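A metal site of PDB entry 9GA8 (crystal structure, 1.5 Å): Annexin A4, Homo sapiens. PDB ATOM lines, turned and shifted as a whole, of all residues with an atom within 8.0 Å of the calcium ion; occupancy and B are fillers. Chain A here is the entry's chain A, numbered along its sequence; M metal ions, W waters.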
ATOM      1  N   TYR A 255     -21.081  20.772  -2.788  1.00  0.00           N
ATOM      2  CA  TYR A 255     -19.888  19.963  -2.666  1.00  0.00           C
ATOM      3  C   TYR A 255     -19.979  18.738  -3.552  1.00  0.00           C
ATOM      4  O   TYR A 255     -19.069  18.473  -4.322  1.00  0.00           O
ATOM      5  CB  TYR A 255     -19.683  19.660  -1.185  1.00  0.00           C
ATOM      6  CG  TYR A 255     -18.502  18.739  -0.928  1.00  0.00           C
ATOM      7  CD1 TYR A 255     -17.211  19.247  -0.907  1.00  0.00           C
ATOM      8  CD2 TYR A 255     -18.682  17.368  -0.790  1.00  0.00           C
ATOM      9  CE1 TYR A 255     -16.111  18.426  -0.687  1.00  0.00           C
ATOM     10  CE2 TYR A 255     -17.593  16.540  -0.565  1.00  0.00           C
ATOM     11  CZ  TYR A 255     -16.307  17.076  -0.511  1.00  0.00           C
ATOM     12  OH  TYR A 255     -15.215  16.269  -0.286  1.00  0.00           O
ATOM     13  N   LYS A 256     -21.106  18.015  -3.483  1.00  0.00           N
ATOM     14  CA  LYS A 256     -21.188  16.771  -4.226  1.00  0.00           C
ATOM     15  C   LYS A 256     -21.225  17.052  -5.723  1.00  0.00           C
ATOM     16  O   LYS A 256     -20.826  16.193  -6.511  1.00  0.00           O
ATOM     17  CB  LYS A 256     -22.377  15.963  -3.704  1.00  0.00           C
ATOM     18  CG  LYS A 256     -22.071  15.419  -2.334  1.00  0.00           C
ATOM     19  CD  LYS A 256     -23.191  14.553  -1.760  1.00  0.00           C
ATOM     20  CE  LYS A 256     -22.720  13.767  -0.578  1.00  0.00           C
ATOM     21  NZ  LYS A 256     -23.846  13.055   0.057  1.00  0.00           N
ATOM     22  N   SER A 257     -21.762  18.212  -6.135  1.00  0.00           N
ATOM     23  CA  SER A 257     -21.863  18.492  -7.554  1.00  0.00           C
ATOM     24  C   SER A 257     -20.489  18.754  -8.177  1.00  0.00           C
ATOM     25  O   SER A 257     -20.401  18.702  -9.397  1.00  0.00           O
ATOM     26  CB  SER A 257     -22.742  19.673  -7.846  1.00  0.00           C
ATOM     27  OG  SER A 257     -22.149  20.908  -7.488  1.00  0.00           O
ATOM     28  N   MET A 258     -19.486  19.074  -7.361  1.00  0.00           N
ATOM     29  CA  MET A 258     -18.192  19.512  -7.889  1.00  0.00           C
ATOM     30  C   MET A 258     -17.028  18.601  -7.501  1.00  0.00           C
ATOM     31  O   MET A 258     -16.036  18.555  -8.221  1.00  0.00           O
ATOM     32  CB  MET A 258     -17.911  20.935  -7.430  1.00  0.00           C
ATOM     33  CG  MET A 258     -18.641  21.959  -8.217  1.00  0.00           C
ATOM     34  SD  MET A 258     -18.417  23.669  -7.663  1.00  0.00           S
ATOM     35  CE  MET A 258     -19.389  23.709  -6.137  1.00  0.00           C
ATOM     36  N   LYS A 259     -17.143  17.872  -6.393  1.00  0.00           N
ATOM     37  CA  LYS A 259     -16.023  17.192  -5.796  1.00  0.00           C
ATOM     38  C   LYS A 259     -15.494  16.060  -6.662  1.00  0.00           C
ATOM     39  O   LYS A 259     -14.300  15.796  -6.635  1.00  0.00           O
ATOM     40  CB  LYS A 259     -16.341  16.654  -4.402  1.00  0.00           C
ATOM     41  CG  LYS A 259     -15.114  16.072  -3.656  1.00  0.00           C
ATOM     42  CD  LYS A 259     -13.894  16.994  -3.420  1.00  0.00           C
ATOM     43  CE  LYS A 259     -12.890  16.354  -2.489  1.00  0.00           C
ATOM     44  NZ  LYS A 259     -11.629  17.099  -2.331  1.00  0.00           N
ATOM     45  N   GLY A 260     -16.322  15.456  -7.502  1.00  0.00           N
ATOM     46  CA  GLY A 260     -15.794  14.382  -8.341  1.00  0.00           C
ATOM     47  C   GLY A 260     -14.897  14.851  -9.507  1.00  0.00           C
ATOM     48  O   GLY A 260     -14.602  16.040  -9.699  1.00  0.00           O
ATOM     49  N   LEU A 261     -14.528  13.865 -10.330  1.00  0.00           N
ATOM     50  CA  LEU A 261     -14.175  14.106 -11.709  1.00  0.00           C
ATOM     51  C   LEU A 261     -15.391  14.736 -12.402  1.00  0.00           C
ATOM     52  O   LEU A 261     -16.478  14.188 -12.356  1.00  0.00           O
ATOM     53  CB  LEU A 261     -13.784  12.801 -12.404  1.00  0.00           C
ATOM     54  CG  LEU A 261     -13.202  12.959 -13.822  1.00  0.00           C
ATOM     55  CD1 LEU A 261     -12.030  13.937 -13.864  1.00  0.00           C
ATOM     56  CD2 LEU A 261     -12.775  11.618 -14.404  1.00  0.00           C
ATOM     57  N   GLY A 262     -15.181  15.884 -13.031  1.00  0.00           N
ATOM     58  CA  GLY A 262     -16.240  16.570 -13.742  1.00  0.00           C
ATOM     59  C   GLY A 262     -17.175  17.316 -12.796  1.00  0.00           C
ATOM     60  O   GLY A 262     -16.823  17.605 -11.633  1.00  0.00           O
ATOM     61  N   THR A 263     -18.348  17.683 -13.313  1.00  0.00           N
ATOM     62  CA  THR A 263     -19.235  18.577 -12.603  1.00  0.00           C
ATOM     63  C   THR A 263     -20.677  18.206 -12.936  1.00  0.00           C
ATOM     64  O   THR A 263     -21.006  18.031 -14.114  1.00  0.00           O
ATOM     65  CB  THR A 263     -19.004  20.001 -13.055  1.00  0.00           C
ATOM     66  OG1 THR A 263     -17.632  20.322 -12.877  1.00  0.00           O
ATOM     67  CG2 THR A 263     -19.842  20.965 -12.240  1.00  0.00           C
ATOM     68  N   ASP A 264     -21.509  18.104 -11.900  1.00  0.00           N
ATOM     69  CA  ASP A 264     -22.942  18.034 -12.100  1.00  0.00           C
ATOM     70  C   ASP A 264     -23.471  19.445 -12.320  1.00  0.00           C
ATOM     71  O   ASP A 264     -23.932  20.104 -11.381  1.00  0.00           O
ATOM     72  CB  ASP A 264     -23.585  17.263 -10.960  1.00  0.00           C
ATOM     73  CG  ASP A 264     -25.101  17.153 -11.005  1.00  0.00           C
ATOM     74  OD1 ASP A 264     -25.700  17.607 -12.019  1.00  0.00           O
ATOM     75  OD2 ASP A 264     -25.684  16.655 -10.028  1.00  0.00           O
ATOM     76  N   PHE A 298     -14.210  26.394  -4.958  1.00  0.00           N
ATOM     77  CA  PHE A 298     -14.701  25.214  -5.615  1.00  0.00           C
ATOM     78  C   PHE A 298     -15.244  25.564  -6.990  1.00  0.00           C
ATOM     79  O   PHE A 298     -14.939  24.920  -7.992  1.00  0.00           O
ATOM     80  CB  PHE A 298     -15.814  24.491  -4.820  1.00  0.00           C
ATOM     81  CG  PHE A 298     -15.292  23.281  -4.057  1.00  0.00           C
ATOM     82  CD1 PHE A 298     -14.352  23.451  -3.059  1.00  0.00           C
ATOM     83  CD2 PHE A 298     -15.860  22.020  -4.215  1.00  0.00           C
ATOM     84  CE1 PHE A 298     -13.821  22.376  -2.385  1.00  0.00           C
ATOM     85  CE2 PHE A 298     -15.362  20.957  -3.476  1.00  0.00           C
ATOM     86  CZ  PHE A 298     -14.336  21.144  -2.565  1.00  0.00           C
ATOM     87  N   GLY A 301     -12.510  26.579  -9.323  1.00  0.00           N
ATOM     88  CA  GLY A 301     -11.708  25.443  -9.724  1.00  0.00           C
ATOM     89  C   GLY A 301     -12.419  24.491 -10.682  1.00  0.00           C
ATOM     90  O   GLY A 301     -11.745  23.718 -11.340  1.00  0.00           O
ATOM     91  N   ASP A 302     -13.760  24.485 -10.736  1.00  0.00           N
ATOM     92  CA  ASP A 302     -14.481  23.475 -11.497  1.00  0.00           C
ATOM     93  C   ASP A 302     -15.199  24.017 -12.715  1.00  0.00           C
ATOM     94  O   ASP A 302     -15.807  23.245 -13.450  1.00  0.00           O
ATOM     95  CB  ASP A 302     -15.532  22.734 -10.658  1.00  0.00           C
ATOM     96  CG  ASP A 302     -15.297  21.248 -10.458  1.00  0.00           C
ATOM     97  OD1 ASP A 302     -14.183  20.876 -10.143  1.00  0.00           O
ATOM     98  OD2 ASP A 302     -16.278  20.480 -10.613  1.00  0.00           O
ATOM     99  N   THR A 303     -15.165  25.330 -12.949  1.00  0.00           N
ATOM    100  CA  THR A 303     -15.878  25.916 -14.055  1.00  0.00           C
ATOM    101  C   THR A 303     -14.925  26.893 -14.747  1.00  0.00           C
ATOM    102  O   THR A 303     -13.931  27.311 -14.167  1.00  0.00           O
ATOM    103  CB  THR A 303     -17.189  26.594 -13.603  1.00  0.00           C
ATOM    104  OG1 THR A 303     -16.882  27.692 -12.733  1.00  0.00           O
ATOM    105  CG2 THR A 303     -18.121  25.622 -12.917  1.00  0.00           C
HETATM  106 CA    CA M   1     -15.061  18.427 -10.287  1.00  0.00          CA
HETATM  107  O   HOH W   1     -12.845  18.409  -9.569  1.00  0.00           O
HETATM  108  O   HOH W   2     -13.978  18.677 -12.340  1.00  0.00           O
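The backbone carbonyl oxygen of Asp 302 sits close to the side-chain hydroxyl of Thr 263.
Of the 14 residues printed, 4 come within 4 Å of the calcium ion.
The nearest printed residue that does not touch the calcium ion is Thr 263 (4.1 Å).
The calcium ion is bound by the backbone carbonyl oxygen (O) of Met 258 (2.3 Å), water W1 (2.3 Å), water W2 (2.3 Å), the backbone carbonyl oxygen (O) of Gly 262 (2.4 Å), the side-chain carboxylate (OD2) of Asp 302 (2.4 Å), the backbone carbonyl oxygen (O) of Gly 260 (2.5 Å) and the side-chain carboxylate (OD1) of Asp 302 (2.6 Å).
The calcium ion has seven donor atoms within binding distance.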
